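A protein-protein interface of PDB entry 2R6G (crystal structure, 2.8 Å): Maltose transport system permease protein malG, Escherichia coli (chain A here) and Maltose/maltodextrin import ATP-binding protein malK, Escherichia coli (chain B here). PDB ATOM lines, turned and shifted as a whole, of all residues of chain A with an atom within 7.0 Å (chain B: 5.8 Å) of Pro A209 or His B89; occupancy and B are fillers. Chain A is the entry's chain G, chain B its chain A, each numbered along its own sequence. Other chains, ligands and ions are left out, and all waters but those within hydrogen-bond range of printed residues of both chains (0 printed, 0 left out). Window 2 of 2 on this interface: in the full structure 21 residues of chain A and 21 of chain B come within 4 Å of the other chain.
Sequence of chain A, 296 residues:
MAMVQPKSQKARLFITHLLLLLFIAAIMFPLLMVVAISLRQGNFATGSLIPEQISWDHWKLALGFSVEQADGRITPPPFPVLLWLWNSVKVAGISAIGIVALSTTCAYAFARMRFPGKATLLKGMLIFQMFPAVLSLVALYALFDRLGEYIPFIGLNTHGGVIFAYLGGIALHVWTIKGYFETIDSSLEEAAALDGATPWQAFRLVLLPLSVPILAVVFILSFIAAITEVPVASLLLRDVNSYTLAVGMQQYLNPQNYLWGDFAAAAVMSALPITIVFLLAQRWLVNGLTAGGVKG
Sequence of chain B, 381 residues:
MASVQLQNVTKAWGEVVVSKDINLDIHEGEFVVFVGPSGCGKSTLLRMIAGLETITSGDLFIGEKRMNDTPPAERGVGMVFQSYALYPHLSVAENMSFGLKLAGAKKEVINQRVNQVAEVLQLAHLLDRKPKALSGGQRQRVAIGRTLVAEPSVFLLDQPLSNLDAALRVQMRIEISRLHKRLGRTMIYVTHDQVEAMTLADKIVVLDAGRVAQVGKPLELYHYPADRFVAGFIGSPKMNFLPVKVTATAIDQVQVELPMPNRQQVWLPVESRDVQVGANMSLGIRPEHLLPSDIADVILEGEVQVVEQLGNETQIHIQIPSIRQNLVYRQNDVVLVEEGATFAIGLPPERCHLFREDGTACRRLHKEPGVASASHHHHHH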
ATOM      1  N   LEU A 188     -24.380  10.792  16.760  1.00  0.00           N
ATOM      2  CA  LEU A 188     -24.032  11.778  17.788  1.00  0.00           C
ATOM      3  C   LEU A 188     -23.676  13.142  17.202  1.00  0.00           C
ATOM      4  O   LEU A 188     -23.918  14.177  17.829  1.00  0.00           O
ATOM      5  CB  LEU A 188     -22.882  11.278  18.676  1.00  0.00           C
ATOM      6  CG  LEU A 188     -23.040  10.075  19.620  1.00  0.00           C
ATOM      7  CD1 LEU A 188     -24.462   9.941  20.156  1.00  0.00           C
ATOM      8  CD2 LEU A 188     -22.585   8.773  18.959  1.00  0.00           C
ATOM      9  N   ALA A 202     -19.042  20.424  17.005  1.00  0.00           N
ATOM     10  CA  ALA A 202     -19.299  18.984  16.993  1.00  0.00           C
ATOM     11  C   ALA A 202     -18.009  18.212  17.236  1.00  0.00           C
ATOM     12  O   ALA A 202     -17.998  17.215  17.958  1.00  0.00           O
ATOM     13  CB  ALA A 202     -19.926  18.567  15.672  1.00  0.00           C
ATOM     14  N   PHE A 203     -16.929  18.692  16.625  1.00  0.00           N
ATOM     15  CA  PHE A 203     -15.597  18.113  16.769  1.00  0.00           C
ATOM     16  C   PHE A 203     -15.072  18.244  18.197  1.00  0.00           C
ATOM     17  O   PHE A 203     -14.606  17.267  18.783  1.00  0.00           O
ATOM     18  CB  PHE A 203     -14.645  18.780  15.771  1.00  0.00           C
ATOM     19  CG  PHE A 203     -13.184  18.590  16.076  1.00  0.00           C
ATOM     20  CD1 PHE A 203     -12.429  19.642  16.587  1.00  0.00           C
ATOM     21  CD2 PHE A 203     -12.558  17.373  15.826  1.00  0.00           C
ATOM     22  CE1 PHE A 203     -11.072  19.481  16.860  1.00  0.00           C
ATOM     23  CE2 PHE A 203     -11.201  17.203  16.094  1.00  0.00           C
ATOM     24  CZ  PHE A 203     -10.458  18.259  16.613  1.00  0.00           C
ATOM     25  N   ARG A 204     -15.166  19.450  18.749  1.00  0.00           N
ATOM     26  CA  ARG A 204     -14.591  19.753  20.055  1.00  0.00           C
ATOM     27  C   ARG A 204     -15.425  19.223  21.223  1.00  0.00           C
ATOM     28  O   ARG A 204     -14.888  18.570  22.116  1.00  0.00           O
ATOM     29  CB  ARG A 204     -14.368  21.263  20.212  1.00  0.00           C
ATOM     30  CG  ARG A 204     -13.366  21.627  21.301  1.00  0.00           C
ATOM     31  CD  ARG A 204     -13.689  22.968  21.943  1.00  0.00           C
ATOM     32  NE  ARG A 204     -12.851  23.216  23.117  1.00  0.00           N
ATOM     33  CZ  ARG A 204     -13.044  24.199  23.997  1.00  0.00           C
ATOM     34  NH1 ARG A 204     -14.058  25.046  23.856  1.00  0.00           N
ATOM     35  NH2 ARG A 204     -12.217  24.331  25.027  1.00  0.00           N
ATOM     36  N   LEU A 205     -16.727  19.506  21.209  1.00  0.00           N
ATOM     37  CA  LEU A 205     -17.598  19.237  22.358  1.00  0.00           C
ATOM     38  C   LEU A 205     -18.232  17.844  22.385  1.00  0.00           C
ATOM     39  O   LEU A 205     -18.585  17.341  23.456  1.00  0.00           O
ATOM     40  CB  LEU A 205     -18.682  20.315  22.480  1.00  0.00           C
ATOM     41  CG  LEU A 205     -18.249  21.679  23.025  1.00  0.00           C
ATOM     42  CD1 LEU A 205     -19.355  22.701  22.831  1.00  0.00           C
ATOM     43  CD2 LEU A 205     -17.851  21.600  24.497  1.00  0.00           C
ATOM     44  N   VAL A 206     -18.381  17.231  21.212  1.00  0.00           N
ATOM     45  CA  VAL A 206     -19.015  15.916  21.109  1.00  0.00           C
ATOM     46  C   VAL A 206     -18.003  14.808  20.815  1.00  0.00           C
ATOM     47  O   VAL A 206     -17.892  13.853  21.584  1.00  0.00           O
ATOM     48  CB  VAL A 206     -20.154  15.896  20.049  1.00  0.00           C
ATOM     49  CG1 VAL A 206     -20.793  14.512  19.962  1.00  0.00           C
ATOM     50  CG2 VAL A 206     -21.205  16.948  20.370  1.00  0.00           C
ATOM     51  N   LEU A 207     -17.267  14.948  19.712  1.00  0.00           N
ATOM     52  CA  LEU A 207     -16.411  13.876  19.206  1.00  0.00           C
ATOM     53  C   LEU A 207     -15.157  13.624  20.043  1.00  0.00           C
ATOM     54  O   LEU A 207     -14.950  12.507  20.521  1.00  0.00           O
ATOM     55  CB  LEU A 207     -16.045  14.118  17.737  1.00  0.00           C
ATOM     56  CG  LEU A 207     -15.317  12.991  16.992  1.00  0.00           C
ATOM     57  CD1 LEU A 207     -16.087  11.676  17.053  1.00  0.00           C
ATOM     58  CD2 LEU A 207     -15.071  13.388  15.552  1.00  0.00           C
ATOM     59  N   LEU A 208     -14.329  14.652  20.219  1.00  0.00           N
ATOM     60  CA  LEU A 208     -13.087  14.525  20.989  1.00  0.00           C
ATOM     61  C   LEU A 208     -13.240  13.792  22.330  1.00  0.00           C
ATOM     62  O   LEU A 208     -12.547  12.799  22.555  1.00  0.00           O
ATOM     63  CB  LEU A 208     -12.401  15.885  21.191  1.00  0.00           C
ATOM     64  CG  LEU A 208     -11.661  16.520  20.011  1.00  0.00           C
ATOM     65  CD1 LEU A 208     -10.829  17.703  20.484  1.00  0.00           C
ATOM     66  CD2 LEU A 208     -10.784  15.503  19.297  1.00  0.00           C
ATOM     67  N   PRO A 209     -14.151  14.261  23.214  1.00  0.00           N
ATOM     68  CA  PRO A 209     -14.272  13.607  24.520  1.00  0.00           C
ATOM     69  C   PRO A 209     -14.670  12.127  24.442  1.00  0.00           C
ATOM     70  O   PRO A 209     -14.492  11.393  25.417  1.00  0.00           O
ATOM     71  CB  PRO A 209     -15.358  14.427  25.229  1.00  0.00           C
ATOM     72  CG  PRO A 209     -16.100  15.097  24.143  1.00  0.00           C
ATOM     73  CD  PRO A 209     -15.095  15.388  23.092  1.00  0.00           C
ATOM     74  N   LEU A 210     -15.196  11.704  23.295  1.00  0.00           N
ATOM     75  CA  LEU A 210     -15.512  10.294  23.062  1.00  0.00           C
ATOM     76  C   LEU A 210     -14.364   9.572  22.351  1.00  0.00           C
ATOM     77  O   LEU A 210     -14.293   8.339  22.360  1.00  0.00           O
ATOM     78  CB  LEU A 210     -16.821  10.149  22.274  1.00  0.00           C
ATOM     79  CG  LEU A 210     -18.111  10.638  22.948  1.00  0.00           C
ATOM     80  CD1 LEU A 210     -19.247  10.722  21.944  1.00  0.00           C
ATOM     81  CD2 LEU A 210     -18.511   9.754  24.122  1.00  0.00           C
ATOM     82  N   SER A 211     -13.468  10.350  21.747  1.00  0.00           N
ATOM     83  CA  SER A 211     -12.302   9.821  21.041  1.00  0.00           C
ATOM     84  C   SER A 211     -11.062   9.879  21.932  1.00  0.00           C
ATOM     85  O   SER A 211      -9.969   9.464  21.535  1.00  0.00           O
ATOM     86  CB  SER A 211     -12.061  10.614  19.755  1.00  0.00           C
ATOM     87  OG  SER A 211     -13.253  10.735  18.995  1.00  0.00           O
ATOM     88  N   VAL A 212     -11.266  10.381  23.147  1.00  0.00           N
ATOM     89  CA  VAL A 212     -10.213  10.628  24.137  1.00  0.00           C
ATOM     90  C   VAL A 212      -9.131   9.531  24.333  1.00  0.00           C
ATOM     91  O   VAL A 212      -7.951   9.870  24.426  1.00  0.00           O
ATOM     92  CB  VAL A 212     -10.843  11.151  25.483  1.00  0.00           C
ATOM     93  CG1 VAL A 212     -10.242  10.505  26.709  1.00  0.00           C
ATOM     94  CG2 VAL A 212     -10.743  12.668  25.563  1.00  0.00           C
ATOM     95  N   PRO A 213      -9.512   8.232  24.390  1.00  0.00           N
ATOM     96  CA  PRO A 213      -8.458   7.218  24.577  1.00  0.00           C
ATOM     97  C   PRO A 213      -7.384   7.184  23.482  1.00  0.00           C
ATOM     98  O   PRO A 213      -6.197   7.096  23.803  1.00  0.00           O
ATOM     99  CB  PRO A 213      -9.229   5.891  24.619  1.00  0.00           C
ATOM    100  CG  PRO A 213     -10.543   6.180  24.019  1.00  0.00           C
ATOM    101  CD  PRO A 213     -10.848   7.612  24.325  1.00  0.00           C
ATOM    102  N   LEU A 215      -6.492   9.598  21.708  1.00  0.00           N
ATOM    103  CA  LEU A 215      -5.753  10.848  21.840  1.00  0.00           C
ATOM    104  C   LEU A 215      -4.599  10.663  22.822  1.00  0.00           C
ATOM    105  O   LEU A 215      -3.514  11.210  22.627  1.00  0.00           O
ATOM    106  CB  LEU A 215      -6.668  11.985  22.305  1.00  0.00           C
ATOM    107  CG  LEU A 215      -7.856  12.452  21.452  1.00  0.00           C
ATOM    108  CD1 LEU A 215      -8.542  13.638  22.122  1.00  0.00           C
ATOM    109  CD2 LEU A 215      -7.439  12.826  20.039  1.00  0.00           C
ATOM    110  N   TRP A 284      -7.431   8.748  30.678  1.00  0.00           N
ATOM    111  CA  TRP A 284      -8.103   8.926  29.395  1.00  0.00           C
ATOM    112  C   TRP A 284      -8.368   7.609  28.671  1.00  0.00           C
ATOM    113  O   TRP A 284      -9.160   7.561  27.728  1.00  0.00           O
ATOM    114  CB  TRP A 284      -7.275   9.862  28.510  1.00  0.00           C
ATOM    115  CG  TRP A 284      -7.550  11.325  28.733  1.00  0.00           C
ATOM    116  CD1 TRP A 284      -8.054  11.910  29.863  1.00  0.00           C
ATOM    117  CD2 TRP A 284      -7.318  12.393  27.801  1.00  0.00           C
ATOM    118  NE1 TRP A 284      -8.163  13.269  29.689  1.00  0.00           N
ATOM    119  CE2 TRP A 284      -7.715  13.595  28.434  1.00  0.00           C
ATOM    120  CE3 TRP A 284      -6.814  12.450  26.490  1.00  0.00           C
ATOM    121  CZ2 TRP A 284      -7.627  14.842  27.801  1.00  0.00           C
ATOM    122  CZ3 TRP A 284      -6.726  13.689  25.862  1.00  0.00           C
ATOM    123  CH2 TRP A 284      -7.132  14.869  26.520  1.00  0.00           C
ATOM    124  N   LEU A 289     -17.106   4.596  26.987  1.00  0.00           N
ATOM    125  CA  LEU A 289     -17.326   6.035  26.865  1.00  0.00           C
ATOM    126  C   LEU A 289     -18.561   6.325  26.030  1.00  0.00           C
ATOM    127  O   LEU A 289     -19.265   7.313  26.260  1.00  0.00           O
ATOM    128  CB  LEU A 289     -16.116   6.713  26.225  1.00  0.00           C
ATOM    129  CG  LEU A 289     -15.006   7.196  27.155  1.00  0.00           C
ATOM    130  CD1 LEU A 289     -13.790   7.588  26.344  1.00  0.00           C
ATOM    131  CD2 LEU A 289     -15.476   8.366  28.016  1.00  0.00           C
ATOM    132  N   THR A 290     -18.814   5.437  25.071  1.00  0.00           N
ATOM    133  CA  THR A 290     -19.893   5.583  24.106  1.00  0.00           C
ATOM    134  C   THR A 290     -21.149   4.787  24.510  1.00  0.00           C
ATOM    135  O   THR A 290     -22.183   4.864  23.841  1.00  0.00           O
ATOM    136  CB  THR A 290     -19.388   5.214  22.679  1.00  0.00           C
ATOM    137  OG1 THR A 290     -20.120   5.951  21.693  1.00  0.00           O
ATOM    138  CG2 THR A 290     -19.482   3.703  22.406  1.00  0.00           C
ATOM    139  N   ALA A 291     -21.049   4.040  25.612  1.00  0.00           N
ATOM    140  CA  ALA A 291     -22.172   3.272  26.168  1.00  0.00           C
ATOM    141  C   ALA A 291     -23.365   4.166  26.498  1.00  0.00           C
ATOM    142  O   ALA A 291     -23.202   5.283  26.999  1.00  0.00           O
ATOM    143  CB  ALA A 291     -21.732   2.495  27.399  1.00  0.00           C
ATOM    144  N   TYR B  87     -25.863  12.169  23.852  1.00  0.00           N
ATOM    145  CA  TYR B  87     -24.431  12.374  24.028  1.00  0.00           C
ATOM    146  C   TYR B  87     -23.979  11.624  25.283  1.00  0.00           C
ATOM    147  O   TYR B  87     -24.262  12.066  26.403  1.00  0.00           O
ATOM    148  CB  TYR B  87     -24.094  13.866  24.121  1.00  0.00           C
ATOM    149  CG  TYR B  87     -24.765  14.743  23.075  1.00  0.00           C
ATOM    150  CD1 TYR B  87     -25.645  15.757  23.454  1.00  0.00           C
ATOM    151  CD2 TYR B  87     -24.516  14.566  21.712  1.00  0.00           C
ATOM    152  CE1 TYR B  87     -26.262  16.567  22.507  1.00  0.00           C
ATOM    153  CE2 TYR B  87     -25.131  15.375  20.756  1.00  0.00           C
ATOM    154  CZ  TYR B  87     -26.001  16.373  21.162  1.00  0.00           C
ATOM    155  OH  TYR B  87     -26.614  17.179  20.230  1.00  0.00           O
ATOM    156  N   PRO B  88     -23.272  10.487  25.099  1.00  0.00           N
ATOM    157  CA  PRO B  88     -22.959   9.561  26.195  1.00  0.00           C
ATOM    158  C   PRO B  88     -22.030  10.171  27.239  1.00  0.00           C
ATOM    159  O   PRO B  88     -22.083   9.793  28.410  1.00  0.00           O
ATOM    160  CB  PRO B  88     -22.253   8.393  25.488  1.00  0.00           C
ATOM    161  CG  PRO B  88     -22.549   8.561  24.034  1.00  0.00           C
ATOM    162  CD  PRO B  88     -22.695  10.028  23.822  1.00  0.00           C
ATOM    163  N   HIS B  89     -21.198  11.112  26.805  1.00  0.00           N
ATOM    164  CA  HIS B  89     -20.223  11.777  27.661  1.00  0.00           C
ATOM    165  C   HIS B  89     -20.829  12.924  28.480  1.00  0.00           C
ATOM    166  O   HIS B  89     -20.130  13.561  29.272  1.00  0.00           O
ATOM    167  CB  HIS B  89     -19.075  12.308  26.802  1.00  0.00           C
ATOM    168  CG  HIS B  89     -19.484  13.397  25.860  1.00  0.00           C
ATOM    169  ND1 HIS B  89     -20.294  13.172  24.768  1.00  0.00           N
ATOM    170  CD2 HIS B  89     -19.200  14.721  25.852  1.00  0.00           C
ATOM    171  CE1 HIS B  89     -20.492  14.310  24.127  1.00  0.00           C
ATOM    172  NE2 HIS B  89     -19.838  15.264  24.763  1.00  0.00           N
ATOM    173  N   LEU B  90     -22.120  13.185  28.280  1.00  0.00           N
ATOM    174  CA  LEU B  90     -22.804  14.289  28.955  1.00  0.00           C
ATOM    175  C   LEU B  90     -24.013  13.808  29.753  1.00  0.00           C
ATOM    176  O   LEU B  90     -24.616  12.787  29.424  1.00  0.00           O
ATOM    177  CB  LEU B  90     -23.231  15.363  27.944  1.00  0.00           C
ATOM    178  CG  LEU B  90     -22.158  16.086  27.119  1.00  0.00           C
ATOM    179  CD1 LEU B  90     -22.799  16.987  26.068  1.00  0.00           C
ATOM    180  CD2 LEU B  90     -21.197  16.886  27.998  1.00  0.00           C
ATOM    181  N   SER B  91     -24.364  14.558  30.795  1.00  0.00           N
ATOM    182  CA  SER B  91     -25.487  14.205  31.662  1.00  0.00           C
ATOM    183  C   SER B  91     -26.836  14.478  30.995  1.00  0.00           C
ATOM    184  O   SER B  91     -26.889  15.023  29.893  1.00  0.00           O
ATOM    185  CB  SER B  91     -25.395  14.962  32.992  1.00  0.00           C
ATOM    186  OG  SER B  91     -25.751  16.324  32.834  1.00  0.00           O
ATOM    187  N   GLU B  94     -27.043  18.183  30.701  1.00  0.00           N
ATOM    188  CA  GLU B  94     -26.142  18.639  29.642  1.00  0.00           C
ATOM    189  C   GLU B  94     -26.602  18.225  28.238  1.00  0.00           C
ATOM    190  O   GLU B  94     -26.268  18.885  27.255  1.00  0.00           O
ATOM    191  CB  GLU B  94     -24.714  18.156  29.912  1.00  0.00           C
ATOM    192  CG  GLU B  94     -24.095  18.750  31.172  1.00  0.00           C
ATOM    193  CD  GLU B  94     -22.727  18.176  31.504  1.00  0.00           C
ATOM    194  OE1 GLU B  94     -22.423  17.039  31.078  1.00  0.00           O
ATOM    195  OE2 GLU B  94     -21.954  18.867  32.201  1.00  0.00           O
ATOM    196  N   LYS B 130     -25.721  10.127  33.385  1.00  0.00           N
ATOM    197  CA  LYS B 130     -25.326   9.994  31.990  1.00  0.00           C
ATOM    198  C   LYS B 130     -26.143   8.843  31.384  1.00  0.00           C
ATOM    199  O   LYS B 130     -26.626   7.980  32.123  1.00  0.00           O
ATOM    200  CB  LYS B 130     -23.815   9.743  31.884  1.00  0.00           C
ATOM    201  CG  LYS B 130     -23.326   8.507  32.627  1.00  0.00           C
ATOM    202  CD  LYS B 130     -21.895   8.663  33.122  1.00  0.00           C
ATOM    203  CE  LYS B 130     -21.541   7.578  34.141  1.00  0.00           C
ATOM    204  NZ  LYS B 130     -22.338   7.690  35.404  1.00  0.00           N
ATOM    205  N   PRO B 131     -26.314   8.830  30.046  1.00  0.00           N
ATOM    206  CA  PRO B 131     -27.172   7.840  29.387  1.00  0.00           C
ATOM    207  C   PRO B 131     -26.980   6.390  29.839  1.00  0.00           C
ATOM    208  O   PRO B 131     -27.973   5.680  30.025  1.00  0.00           O
ATOM    209  CB  PRO B 131     -26.800   7.991  27.912  1.00  0.00           C
ATOM    210  CG  PRO B 131     -26.429   9.417  27.789  1.00  0.00           C
ATOM    211  CD  PRO B 131     -25.719   9.759  29.068  1.00  0.00           C
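A ring nitrogen (NE2) of His B89 lies within hydrogen-bond range of the backbone carbonyl oxygen of Leu A205 (2.8 Å).
Tyr B87 touches Leu A188 (CE2 to O, 3.4 Å). Val A206 touches His B89. His B89 touches Pro A209 (CD2 to CG, 3.6 Å). Leu A210 touches Pro B88 (CD1 to CD, 3.99 Å). Leu A210 touches His B89. O of Leu A289 touches CB of Pro B88 (3.3 Å). Pro B88 touches Thr A290 (CG to O, 3.7 Å). Pro B88 touches Ala A291 (CB to O, 3.6 Å).
Printed residues of chain B within 4 Å of Val A206: His B89 (3.7 Å). Printed residues of chain B within 4 Å of Leu A289: Pro B88. Printed residues of chain A within 4 Å of Tyr B87: Leu A188. Of the printed residues of chain A, Pro B88 touches Leu A210 (3.99 Å), Leu A289 (3.3 Å), Thr A290 (3.7 Å) and Ala A291 (3.6 Å). The nearest residue of chain A that does not touch His B89 is Leu A289 (4.3 Å).
Of the 8 printed residues of chain B, 3 touch a printed residue of chain A. Printed residues of chain B that touch a printed residue of chain A: Tyr B87, Pro B88 and His B89. Hydrophobic or aromatic side chains of chain B that line the printed part of chain A: Tyr B87, Pro B88 and His B89. Of the 18 printed residues of chain A, 8 touch a printed residue of chain B. Hydrophobic or aromatic side chains of chain A that line the printed part of chain B: Pro A209 and Leu A210. Among the printed residues, 9 pairs touch across the chains.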
